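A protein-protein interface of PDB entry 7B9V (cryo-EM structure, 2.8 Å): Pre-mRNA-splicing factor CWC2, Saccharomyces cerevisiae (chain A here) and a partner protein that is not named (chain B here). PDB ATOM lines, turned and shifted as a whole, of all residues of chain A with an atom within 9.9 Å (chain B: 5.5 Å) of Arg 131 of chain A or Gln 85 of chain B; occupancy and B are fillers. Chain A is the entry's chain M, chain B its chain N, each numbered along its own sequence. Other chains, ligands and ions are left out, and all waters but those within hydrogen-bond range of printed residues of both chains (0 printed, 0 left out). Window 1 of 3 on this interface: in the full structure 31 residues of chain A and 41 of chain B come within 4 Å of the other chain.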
ATOM      1  N   THR A 106      28.873 -23.084 -24.655  1.00  0.00           N
ATOM      2  CA  THR A 106      28.092 -24.228 -24.140  1.00  0.00           C
ATOM      3  C   THR A 106      26.859 -23.860 -23.304  1.00  0.00           C
ATOM      4  O   THR A 106      25.919 -24.661 -23.226  1.00  0.00           O
ATOM      5  CB  THR A 106      29.019 -25.182 -23.343  1.00  0.00           C
ATOM      6  OG1 THR A 106      28.391 -26.460 -23.197  1.00  0.00           O
ATOM      7  CG2 THR A 106      29.439 -24.637 -21.955  1.00  0.00           C
ATOM      8  N   GLU A 107      26.858 -22.693 -22.642  1.00  0.00           N
ATOM      9  CA  GLU A 107      25.723 -22.268 -21.820  1.00  0.00           C
ATOM     10  C   GLU A 107      24.455 -22.039 -22.640  1.00  0.00           C
ATOM     11  O   GLU A 107      23.355 -22.369 -22.192  1.00  0.00           O
ATOM     12  CB  GLU A 107      26.096 -20.997 -21.051  1.00  0.00           C
ATOM     13  CG  GLU A 107      27.158 -21.190 -19.969  1.00  0.00           C
ATOM     14  CD  GLU A 107      26.749 -22.116 -18.817  1.00  0.00           C
ATOM     15  OE1 GLU A 107      25.545 -22.382 -18.593  1.00  0.00           O
ATOM     16  OE2 GLU A 107      27.666 -22.628 -18.142  1.00  0.00           O
ATOM     17  N   VAL A 108      24.592 -21.496 -23.839  1.00  0.00           N
ATOM     18  CA  VAL A 108      23.456 -21.204 -24.701  1.00  0.00           C
ATOM     19  C   VAL A 108      23.414 -22.053 -25.964  1.00  0.00           C
ATOM     20  O   VAL A 108      22.356 -22.100 -26.619  1.00  0.00           O
ATOM     21  CB  VAL A 108      23.391 -19.706 -25.058  1.00  0.00           C
ATOM     22  CG1 VAL A 108      23.142 -18.875 -23.804  1.00  0.00           C
ATOM     23  CG2 VAL A 108      24.654 -19.282 -25.759  1.00  0.00           C
ATOM     24  N   LEU A 109      24.501 -22.732 -26.321  1.00  0.00           N
ATOM     25  CA  LEU A 109      24.557 -23.560 -27.512  1.00  0.00           C
ATOM     26  C   LEU A 109      24.802 -25.026 -27.173  1.00  0.00           C
ATOM     27  O   LEU A 109      25.465 -25.374 -26.189  1.00  0.00           O
ATOM     28  CB  LEU A 109      25.640 -23.072 -28.479  1.00  0.00           C
ATOM     29  CG  LEU A 109      25.512 -21.646 -29.018  1.00  0.00           C
ATOM     30  CD1 LEU A 109      26.475 -21.464 -30.140  1.00  0.00           C
ATOM     31  CD2 LEU A 109      24.132 -21.369 -29.552  1.00  0.00           C
ATOM     32  N   LYS A 116      19.928 -23.288 -27.675  1.00  0.00           N
ATOM     33  CA  LYS A 116      19.073 -23.888 -26.654  1.00  0.00           C
ATOM     34  C   LYS A 116      17.821 -23.053 -26.364  1.00  0.00           C
ATOM     35  O   LYS A 116      17.700 -21.891 -26.746  1.00  0.00           O
ATOM     36  CB  LYS A 116      19.872 -24.087 -25.372  1.00  0.00           C
ATOM     37  CG  LYS A 116      20.850 -25.213 -25.489  1.00  0.00           C
ATOM     38  CD  LYS A 116      21.828 -25.258 -24.345  1.00  0.00           C
ATOM     39  CE  LYS A 116      22.709 -26.462 -24.566  1.00  0.00           C
ATOM     40  NZ  LYS A 116      23.979 -26.507 -23.798  1.00  0.00           N
ATOM     41  N   PHE A 117      16.872 -23.686 -25.669  1.00  0.00           N
ATOM     42  CA  PHE A 117      15.588 -23.084 -25.317  1.00  0.00           C
ATOM     43  C   PHE A 117      15.448 -22.761 -23.829  1.00  0.00           C
ATOM     44  O   PHE A 117      16.262 -23.157 -23.002  1.00  0.00           O
ATOM     45  CB  PHE A 117      14.470 -24.004 -25.791  1.00  0.00           C
ATOM     46  CG  PHE A 117      14.240 -23.929 -27.269  1.00  0.00           C
ATOM     47  CD1 PHE A 117      15.065 -24.629 -28.146  1.00  0.00           C
ATOM     48  CD2 PHE A 117      13.232 -23.133 -27.780  1.00  0.00           C
ATOM     49  CE1 PHE A 117      14.874 -24.551 -29.497  1.00  0.00           C
ATOM     50  CE2 PHE A 117      13.034 -23.059 -29.141  1.00  0.00           C
ATOM     51  CZ  PHE A 117      13.862 -23.761 -29.992  1.00  0.00           C
ATOM     52  N   ALA A 118      14.431 -21.956 -23.495  1.00  0.00           N
ATOM     53  CA  ALA A 118      14.102 -21.730 -22.085  1.00  0.00           C
ATOM     54  C   ALA A 118      13.486 -22.962 -21.427  1.00  0.00           C
ATOM     55  O   ALA A 118      13.984 -23.460 -20.408  1.00  0.00           O
ATOM     56  CB  ALA A 118      13.164 -20.530 -21.945  1.00  0.00           C
ATOM     57  N   ASP A 119      12.404 -23.470 -22.010  1.00  0.00           N
ATOM     58  CA  ASP A 119      11.670 -24.620 -21.504  1.00  0.00           C
ATOM     59  C   ASP A 119      11.961 -25.824 -22.387  1.00  0.00           C
ATOM     60  O   ASP A 119      12.103 -25.679 -23.605  1.00  0.00           O
ATOM     61  CB  ASP A 119      10.157 -24.358 -21.514  1.00  0.00           C
ATOM     62  CG  ASP A 119       9.776 -23.026 -20.898  1.00  0.00           C
ATOM     63  OD1 ASP A 119      10.491 -22.538 -19.997  1.00  0.00           O
ATOM     64  OD2 ASP A 119       8.746 -22.468 -21.324  1.00  0.00           O
ATOM     65  N   TYR A 120      12.117 -26.999 -21.771  1.00  0.00           N
ATOM     66  CA  TYR A 120      12.054 -28.253 -22.519  1.00  0.00           C
ATOM     67  C   TYR A 120      10.722 -28.404 -23.252  1.00  0.00           C
ATOM     68  O   TYR A 120       9.695 -27.854 -22.838  1.00  0.00           O
ATOM     69  CB  TYR A 120      12.217 -29.447 -21.575  1.00  0.00           C
ATOM     70  CG  TYR A 120      13.626 -29.717 -21.119  1.00  0.00           C
ATOM     71  CD1 TYR A 120      14.541 -30.304 -21.985  1.00  0.00           C
ATOM     72  CD2 TYR A 120      14.037 -29.383 -19.832  1.00  0.00           C
ATOM     73  CE1 TYR A 120      15.822 -30.575 -21.576  1.00  0.00           C
ATOM     74  CE2 TYR A 120      15.329 -29.633 -19.420  1.00  0.00           C
ATOM     75  CZ  TYR A 120      16.209 -30.231 -20.300  1.00  0.00           C
ATOM     76  OH  TYR A 120      17.495 -30.463 -19.922  1.00  0.00           O
ATOM     77  N   ILE A 127      16.652 -30.053 -28.324  1.00  0.00           N
ATOM     78  CA  ILE A 127      18.032 -29.618 -28.072  1.00  0.00           C
ATOM     79  C   ILE A 127      18.328 -29.489 -26.575  1.00  0.00           C
ATOM     80  O   ILE A 127      19.435 -29.834 -26.130  1.00  0.00           O
ATOM     81  CB  ILE A 127      18.254 -28.295 -28.842  1.00  0.00           C
ATOM     82  CG1 ILE A 127      18.181 -28.527 -30.352  1.00  0.00           C
ATOM     83  CG2 ILE A 127      19.598 -27.638 -28.537  1.00  0.00           C
ATOM     84  CD1 ILE A 127      17.756 -27.301 -31.134  1.00  0.00           C
ATOM     85  N   GLY A 128      17.362 -29.071 -25.773  1.00  0.00           N
ATOM     86  CA  GLY A 128      17.510 -28.917 -24.339  1.00  0.00           C
ATOM     87  C   GLY A 128      17.483 -27.467 -23.885  1.00  0.00           C
ATOM     88  O   GLY A 128      17.447 -26.525 -24.677  1.00  0.00           O
ATOM     89  N   SER A 129      17.491 -27.316 -22.560  1.00  0.00           N
ATOM     90  CA  SER A 129      17.306 -26.035 -21.889  1.00  0.00           C
ATOM     91  C   SER A 129      18.622 -25.403 -21.453  1.00  0.00           C
ATOM     92  O   SER A 129      19.497 -26.079 -20.909  1.00  0.00           O
ATOM     93  CB  SER A 129      16.382 -26.204 -20.679  1.00  0.00           C
ATOM     94  OG  SER A 129      16.260 -25.006 -19.937  1.00  0.00           O
ATOM     95  N   PHE A 130      18.755 -24.087 -21.679  1.00  0.00           N
ATOM     96  CA  PHE A 130      19.887 -23.352 -21.111  1.00  0.00           C
ATOM     97  C   PHE A 130      19.805 -23.153 -19.593  1.00  0.00           C
ATOM     98  O   PHE A 130      20.807 -22.755 -18.990  1.00  0.00           O
ATOM     99  CB  PHE A 130      20.106 -22.004 -21.842  1.00  0.00           C
ATOM    100  CG  PHE A 130      18.879 -21.104 -21.978  1.00  0.00           C
ATOM    101  CD1 PHE A 130      18.303 -20.457 -20.886  1.00  0.00           C
ATOM    102  CD2 PHE A 130      18.414 -20.783 -23.249  1.00  0.00           C
ATOM    103  CE1 PHE A 130      17.216 -19.610 -21.053  1.00  0.00           C
ATOM    104  CE2 PHE A 130      17.336 -19.927 -23.426  1.00  0.00           C
ATOM    105  CZ  PHE A 130      16.746 -19.335 -22.328  1.00  0.00           C
ATOM    106  N   ARG A 131      18.652 -23.399 -18.968  1.00  0.00           N
ATOM    107  CA  ARG A 131      18.515 -23.301 -17.514  1.00  0.00           C
ATOM    108  C   ARG A 131      19.077 -24.510 -16.760  1.00  0.00           C
ATOM    109  O   ARG A 131      19.643 -24.344 -15.672  1.00  0.00           O
ATOM    110  CB  ARG A 131      17.049 -23.071 -17.141  1.00  0.00           C
ATOM    111  CG  ARG A 131      16.483 -21.740 -17.639  1.00  0.00           C
ATOM    112  CD  ARG A 131      15.070 -21.518 -17.129  1.00  0.00           C
ATOM    113  NE  ARG A 131      14.439 -20.355 -17.748  1.00  0.00           N
ATOM    114  CZ  ARG A 131      13.205 -20.341 -18.234  1.00  0.00           C
ATOM    115  NH1 ARG A 131      12.476 -21.449 -18.306  1.00  0.00           N
ATOM    116  NH2 ARG A 131      12.698 -19.195 -18.680  1.00  0.00           N
ATOM    117  N   LYS A 132      18.928 -25.726 -17.300  1.00  0.00           N
ATOM    118  CA  LYS A 132      19.163 -26.962 -16.546  1.00  0.00           C
ATOM    119  C   LYS A 132      20.624 -27.431 -16.512  1.00  0.00           C
ATOM    120  O   LYS A 132      21.095 -27.828 -15.439  1.00  0.00           O
ATOM    121  CB  LYS A 132      18.260 -28.069 -17.106  1.00  0.00           C
ATOM    122  CG  LYS A 132      18.346 -29.422 -16.405  1.00  0.00           C
ATOM    123  CD  LYS A 132      17.972 -29.332 -14.923  1.00  0.00           C
ATOM    124  CE  LYS A 132      18.076 -30.705 -14.269  1.00  0.00           C
ATOM    125  NZ  LYS A 132      16.907 -31.582 -14.579  1.00  0.00           N
ATOM    126  N   LYS A 133      21.340 -27.410 -17.654  1.00  0.00           N
ATOM    127  CA  LYS A 133      22.677 -28.043 -17.859  1.00  0.00           C
ATOM    128  C   LYS A 133      22.658 -29.570 -17.583  1.00  0.00           C
ATOM    129  O   LYS A 133      23.359 -30.110 -16.722  1.00  0.00           O
ATOM    130  CB  LYS A 133      23.790 -27.274 -17.102  1.00  0.00           C
ATOM    131  CG  LYS A 133      25.275 -27.691 -17.374  1.00  0.00           C
ATOM    132  CD  LYS A 133      26.249 -26.522 -17.494  1.00  0.00           C
ATOM    133  CE  LYS A 133      26.400 -25.737 -16.215  1.00  0.00           C
ATOM    134  NZ  LYS A 133      27.532 -24.790 -16.358  1.00  0.00           N
ATOM    135  N   ASN A 134      21.697 -30.237 -18.217  1.00  0.00           N
ATOM    136  CA  ASN A 134      21.445 -31.672 -18.065  1.00  0.00           C
ATOM    137  C   ASN A 134      22.519 -32.524 -18.755  1.00  0.00           C
ATOM    138  O   ASN A 134      22.899 -32.263 -19.898  1.00  0.00           O
ATOM    139  CB  ASN A 134      20.079 -31.974 -18.676  1.00  0.00           C
ATOM    140  CG  ASN A 134      19.494 -33.316 -18.265  1.00  0.00           C
ATOM    141  OD1 ASN A 134      20.160 -34.191 -17.725  1.00  0.00           O
ATOM    142  ND2 ASN A 134      18.209 -33.469 -18.538  1.00  0.00           N
ATOM    143  N   GLN A 189      28.165 -32.366 -20.602  1.00  0.00           N
ATOM    144  CA  GLN A 189      26.906 -32.167 -21.330  1.00  0.00           C
ATOM    145  C   GLN A 189      27.071 -32.273 -22.851  1.00  0.00           C
ATOM    146  O   GLN A 189      26.168 -32.775 -23.534  1.00  0.00           O
ATOM    147  CB  GLN A 189      26.287 -30.801 -20.962  1.00  0.00           C
ATOM    148  CG  GLN A 189      24.980 -30.480 -21.721  1.00  0.00           C
ATOM    149  CD  GLN A 189      24.222 -29.248 -21.283  1.00  0.00           C
ATOM    150  OE1 GLN A 189      24.799 -28.248 -20.886  1.00  0.00           O
ATOM    151  NE2 GLN A 189      22.907 -29.320 -21.401  1.00  0.00           N
ATOM    152  N   LEU A 242      26.294 -30.370  -5.845  1.00  0.00           N
ATOM    153  CA  LEU A 242      25.962 -28.943  -5.925  1.00  0.00           C
ATOM    154  C   LEU A 242      26.748 -28.133  -4.899  1.00  0.00           C
ATOM    155  O   LEU A 242      27.242 -27.038  -5.213  1.00  0.00           O
ATOM    156  CB  LEU A 242      24.459 -28.728  -5.729  1.00  0.00           C
ATOM    157  CG  LEU A 242      23.913 -27.304  -5.894  1.00  0.00           C
ATOM    158  CD1 LEU A 242      24.071 -26.793  -7.319  1.00  0.00           C
ATOM    159  CD2 LEU A 242      22.452 -27.235  -5.462  1.00  0.00           C
ATOM    160  N   GLU A 245      30.426 -27.986  -6.114  1.00  0.00           N
ATOM    161  CA  GLU A 245      30.543 -27.001  -7.191  1.00  0.00           C
ATOM    162  C   GLU A 245      30.511 -25.571  -6.653  1.00  0.00           C
ATOM    163  O   GLU A 245      31.285 -24.708  -7.104  1.00  0.00           O
ATOM    164  CB  GLU A 245      29.429 -27.214  -8.224  1.00  0.00           C
ATOM    165  CG  GLU A 245      29.421 -26.187  -9.358  1.00  0.00           C
ATOM    166  CD  GLU A 245      28.434 -26.518 -10.457  1.00  0.00           C
ATOM    167  OE1 GLU A 245      27.262 -26.813 -10.144  1.00  0.00           O
ATOM    168  OE2 GLU A 245      28.835 -26.468 -11.640  1.00  0.00           O
ATOM    169  N   SER A 246      29.640 -25.322  -5.662  1.00  0.00           N
ATOM    170  CA  SER A 246      29.556 -24.007  -5.027  1.00  0.00           C
ATOM    171  C   SER A 246      30.855 -23.654  -4.313  1.00  0.00           C
ATOM    172  O   SER A 246      31.335 -22.514  -4.414  1.00  0.00           O
ATOM    173  CB  SER A 246      28.381 -23.989  -4.048  1.00  0.00           C
ATOM    174  OG  SER A 246      28.133 -22.693  -3.543  1.00  0.00           O
ATOM    175  N   MET A 249      33.509 -22.765  -6.635  1.00  0.00           N
ATOM    176  CA  MET A 249      33.308 -21.467  -7.274  1.00  0.00           C
ATOM    177  C   MET A 249      33.649 -20.311  -6.342  1.00  0.00           C
ATOM    178  O   MET A 249      34.079 -19.242  -6.832  1.00  0.00           O
ATOM    179  CB  MET A 249      31.872 -21.369  -7.817  1.00  0.00           C
ATOM    180  CG  MET A 249      31.545 -20.070  -8.551  1.00  0.00           C
ATOM    181  SD  MET A 249      32.765 -19.724  -9.830  1.00  0.00           S
ATOM    182  CE  MET A 249      32.524 -21.091 -10.948  1.00  0.00           C
ATOM    183  N   ILE B  36      13.729 -15.776 -23.598  1.00  0.00           N
ATOM    184  CA  ILE B  36      13.015 -15.739 -22.312  1.00  0.00           C
ATOM    185  C   ILE B  36      11.572 -15.261 -22.440  1.00  0.00           C
ATOM    186  O   ILE B  36      10.649 -15.922 -21.951  1.00  0.00           O
ATOM    187  CB  ILE B  36      13.794 -14.897 -21.271  1.00  0.00           C
ATOM    188  CG1 ILE B  36      15.127 -15.558 -20.939  1.00  0.00           C
ATOM    189  CG2 ILE B  36      12.995 -14.705 -19.992  1.00  0.00           C
ATOM    190  CD1 ILE B  36      16.096 -14.650 -20.221  1.00  0.00           C
ATOM    191  N   PRO B  83      26.754 -18.886 -14.092  1.00  0.00           N
ATOM    192  CA  PRO B  83      25.344 -19.069 -14.465  1.00  0.00           C
ATOM    193  C   PRO B  83      24.404 -18.781 -13.296  1.00  0.00           C
ATOM    194  O   PRO B  83      24.806 -18.855 -12.133  1.00  0.00           O
ATOM    195  CB  PRO B  83      25.258 -20.528 -14.932  1.00  0.00           C
ATOM    196  CG  PRO B  83      26.282 -21.213 -14.204  1.00  0.00           C
ATOM    197  CD  PRO B  83      27.418 -20.200 -14.099  1.00  0.00           C
ATOM    198  N   ILE B  84      23.162 -18.384 -13.649  1.00  0.00           N
ATOM    199  CA  ILE B  84      22.110 -17.930 -12.711  1.00  0.00           C
ATOM    200  C   ILE B  84      21.874 -18.914 -11.561  1.00  0.00           C
ATOM    201  O   ILE B  84      21.739 -18.493 -10.404  1.00  0.00           O
ATOM    202  CB  ILE B  84      20.797 -17.661 -13.487  1.00  0.00           C
ATOM    203  CG1 ILE B  84      20.947 -16.514 -14.486  1.00  0.00           C
ATOM    204  CG2 ILE B  84      19.601 -17.373 -12.571  1.00  0.00           C
ATOM    205  CD1 ILE B  84      19.734 -16.346 -15.399  1.00  0.00           C
ATOM    206  N   GLN B  85      21.782 -20.218 -11.861  1.00  0.00           N
ATOM    207  CA  GLN B  85      21.480 -21.237 -10.845  1.00  0.00           C
ATOM    208  C   GLN B  85      22.560 -21.284  -9.767  1.00  0.00           C
ATOM    209  O   GLN B  85      22.264 -21.243  -8.567  1.00  0.00           O
ATOM    210  CB  GLN B  85      21.293 -22.609 -11.497  1.00  0.00           C
ATOM    211  CG  GLN B  85      20.239 -22.693 -12.616  1.00  0.00           C
ATOM    212  CD  GLN B  85      18.875 -22.076 -12.259  1.00  0.00           C
ATOM    213  OE1 GLN B  85      18.389 -22.192 -11.135  1.00  0.00           O
ATOM    214  NE2 GLN B  85      18.276 -21.403 -13.227  1.00  0.00           N
ATOM    215  N   LEU B  86      23.825 -21.304 -10.200  1.00  0.00           N
ATOM    216  CA  LEU B  86      24.980 -21.325  -9.306  1.00  0.00           C
ATOM    217  C   LEU B  86      25.104 -20.020  -8.521  1.00  0.00           C
ATOM    218  O   LEU B  86      25.453 -20.041  -7.335  1.00  0.00           O
ATOM    219  CB  LEU B  86      26.252 -21.616 -10.104  1.00  0.00           C
ATOM    220  CG  LEU B  86      27.578 -21.663  -9.351  1.00  0.00           C
ATOM    221  CD1 LEU B  86      27.546 -22.712  -8.250  1.00  0.00           C
ATOM    222  CD2 LEU B  86      28.683 -21.980 -10.337  1.00  0.00           C
ATOM    223  N   ARG B  87      24.840 -18.884  -9.176  1.00  0.00           N
ATOM    224  CA  ARG B  87      24.842 -17.572  -8.518  1.00  0.00           C
ATOM    225  C   ARG B  87      23.800 -17.481  -7.409  1.00  0.00           C
ATOM    226  O   ARG B  87      24.113 -17.054  -6.289  1.00  0.00           O
ATOM    227  CB  ARG B  87      24.590 -16.461  -9.527  1.00  0.00           C
ATOM    228  CG  ARG B  87      24.717 -15.091  -8.892  1.00  0.00           C
ATOM    229  CD  ARG B  87      24.081 -14.045  -9.756  1.00  0.00           C
ATOM    230  NE  ARG B  87      22.633 -14.234  -9.841  1.00  0.00           N
ATOM    231  CZ  ARG B  87      21.857 -13.655 -10.746  1.00  0.00           C
ATOM    232  NH1 ARG B  87      22.336 -12.748 -11.586  1.00  0.00           N
ATOM    233  NH2 ARG B  87      20.570 -13.970 -10.787  1.00  0.00           N
ATOM    234  N   ASP B  88      22.545 -17.807  -7.725  1.00  0.00           N
ATOM    235  CA  ASP B  88      21.464 -17.742  -6.744  1.00  0.00           C
ATOM    236  C   ASP B  88      21.684 -18.751  -5.621  1.00  0.00           C
ATOM    237  O   ASP B  88      21.287 -18.493  -4.480  1.00  0.00           O
ATOM    238  CB  ASP B  88      20.112 -17.967  -7.417  1.00  0.00           C
ATOM    239  CG  ASP B  88      19.804 -16.921  -8.468  1.00  0.00           C
ATOM    240  OD1 ASP B  88      20.567 -15.938  -8.567  1.00  0.00           O
ATOM    241  OD2 ASP B  88      18.796 -17.076  -9.194  1.00  0.00           O
ATOM    242  N   HIS B  89      22.284 -19.906  -5.930  1.00  0.00           N
ATOM    243  CA  HIS B  89      22.646 -20.870  -4.894  1.00  0.00           C
ATOM    244  C   HIS B  89      23.722 -20.311  -3.969  1.00  0.00           C
ATOM    245  O   HIS B  89      23.664 -20.528  -2.751  1.00  0.00           O
ATOM    246  CB  HIS B  89      23.115 -22.180  -5.524  1.00  0.00           C
ATOM    247  CG  HIS B  89      23.543 -23.198  -4.516  1.00  0.00           C
ATOM    248  ND1 HIS B  89      22.704 -23.664  -3.528  1.00  0.00           N
ATOM    249  CD2 HIS B  89      24.720 -23.844  -4.347  1.00  0.00           C
ATOM    250  CE1 HIS B  89      23.352 -24.544  -2.784  1.00  0.00           C
ATOM    251  NE2 HIS B  89      24.574 -24.675  -3.263  1.00  0.00           N
ATOM    252  N   LEU B  90      24.744 -19.650  -4.533  1.00  0.00           N
ATOM    253  CA  LEU B  90      25.844 -19.074  -3.753  1.00  0.00           C
ATOM    254  C   LEU B  90      25.355 -17.999  -2.788  1.00  0.00           C
ATOM    255  O   LEU B  90      25.766 -17.970  -1.619  1.00  0.00           O
ATOM    256  CB  LEU B  90      26.918 -18.503  -4.679  1.00  0.00           C
ATOM    257  CG  LEU B  90      27.964 -19.463  -5.226  1.00  0.00           C
ATOM    258  CD1 LEU B  90      28.542 -18.946  -6.517  1.00  0.00           C
ATOM    259  CD2 LEU B  90      29.053 -19.569  -4.210  1.00  0.00           C
ATOM    260  N   MET B 100      15.756 -17.058  -5.359  1.00  0.00           N
ATOM    261  CA  MET B 100      15.959 -17.771  -6.613  1.00  0.00           C
ATOM    262  C   MET B 100      15.211 -17.034  -7.716  1.00  0.00           C
ATOM    263  O   MET B 100      14.214 -16.356  -7.465  1.00  0.00           O
ATOM    264  CB  MET B 100      15.458 -19.238  -6.573  1.00  0.00           C
ATOM    265  CG  MET B 100      16.158 -20.194  -5.577  1.00  0.00           C
ATOM    266  SD  MET B 100      15.589 -21.899  -5.521  1.00  0.00           S
ATOM    267  CE  MET B 100      16.306 -22.483  -7.056  1.00  0.00           C
ATOM    268  N   GLU B 103      11.063 -18.185 -12.866  1.00  0.00           N
ATOM    269  CA  GLU B 103      10.840 -18.026 -14.295  1.00  0.00           C
ATOM    270  C   GLU B 103       9.441 -18.459 -14.705  1.00  0.00           C
ATOM    271  O   GLU B 103       8.949 -19.503 -14.262  1.00  0.00           O
ATOM    272  CB  GLU B 103      11.892 -18.807 -15.086  1.00  0.00           C
ATOM    273  CG  GLU B 103      13.347 -18.313 -14.934  1.00  0.00           C
ATOM    274  CD  GLU B 103      13.694 -16.966 -15.610  1.00  0.00           C
ATOM    275  OE1 GLU B 103      12.817 -16.200 -16.081  1.00  0.00           O
ATOM    276  OE2 GLU B 103      14.906 -16.666 -15.662  1.00  0.00           O
ATOM    277  N   ALA B 104       8.800 -17.634 -15.527  1.00  0.00           N
ATOM    278  CA  ALA B 104       7.461 -17.908 -16.026  1.00  0.00           C
ATOM    279  C   ALA B 104       7.425 -19.111 -16.963  1.00  0.00           C
ATOM    280  O   ALA B 104       8.334 -19.320 -17.768  1.00  0.00           O
ATOM    281  CB  ALA B 104       6.944 -16.685 -16.762  1.00  0.00           C
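OE1 of Glu 103 of chain B lies within salt-bridge range of NH2 of Arg 131 of chain A, at 3.97 Å.
O of Ala 118 of chain A sits at hydrogen-bond distance from NH1 of Arg 131 of chain A, at 3.3 Å.
The side-chain carboxylate (OD1) of Asp 119 of chain A is in salt-bridge range of the guanidinium group (NH1) of Arg 131 of chain A (2.8 Å).
OG of Ser 129 of chain A lies within hydrogen-bond range of N of Arg 131 of chain A, 3.0 Å away.
Of the printed residues of chain B, Arg 131 of chain A touches Gln 85 (3.5 Å) and Glu 103 (3.6 Å).
Gln 85 of chain B touches just one residue of chain A: Arg 131 (3.5 Å).
Of the printed residues of chain A, His 89 of chain B touches Leu 242 (3.8 Å) and Ser 246 (3.7 Å).
Of the printed residues of chain B, Met 249 of chain A touches Leu 86 and Leu 90.
Printed residues of chain A within 4 Å of Leu 86 of chain B: Met 249.
The nearest residue of chain A that does not touch Gln 85 of chain B is Lys 132 of chain A (5.7 Å).
The nearest printed residue of chain B that does not touch Ser 246 of chain A is Leu 86 of chain B (4.01 Å).
Arg 131 of chain A touches Gln 85 of chain B.
His 89 of chain B touches Leu 242 of chain A.
Ser 246 of chain A touches His 89 of chain B (CB to CD2, 3.7 Å).
OG of Ser 246 of chain A touches CD2 of Leu 90 of chain B (3.3 Å).
CG of Met 249 of chain A touches CD2 of Leu 86 of chain B, 3.9 Å away.
Leu 90 of chain B touches Met 249 of chain A (CD1 to CG, 3.8 Å).
Printed residues of chain A that touch a printed residue of chain B: Arg 131, Leu 242, Ser 246 and Met 249.
Hydrophobic or aromatic side chains of chain A that line the printed part of chain B: Leu 242 and Met 249.
Of the 12 printed residues of chain B, 5 touch a printed residue of chain A.
Printed residues of chain B that touch a printed residue of chain A: Gln 85, Leu 86, His 89, Leu 90 and Glu 103.
Among the printed residues, 7 pairs touch across the chains.
Among the printed residues, Asp or Glu carboxylates within 4 Å of a Lys or Arg side-chain nitrogen of the other chain: Arg 131 of chain A with Glu 103 of chain B (3.97 Å).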
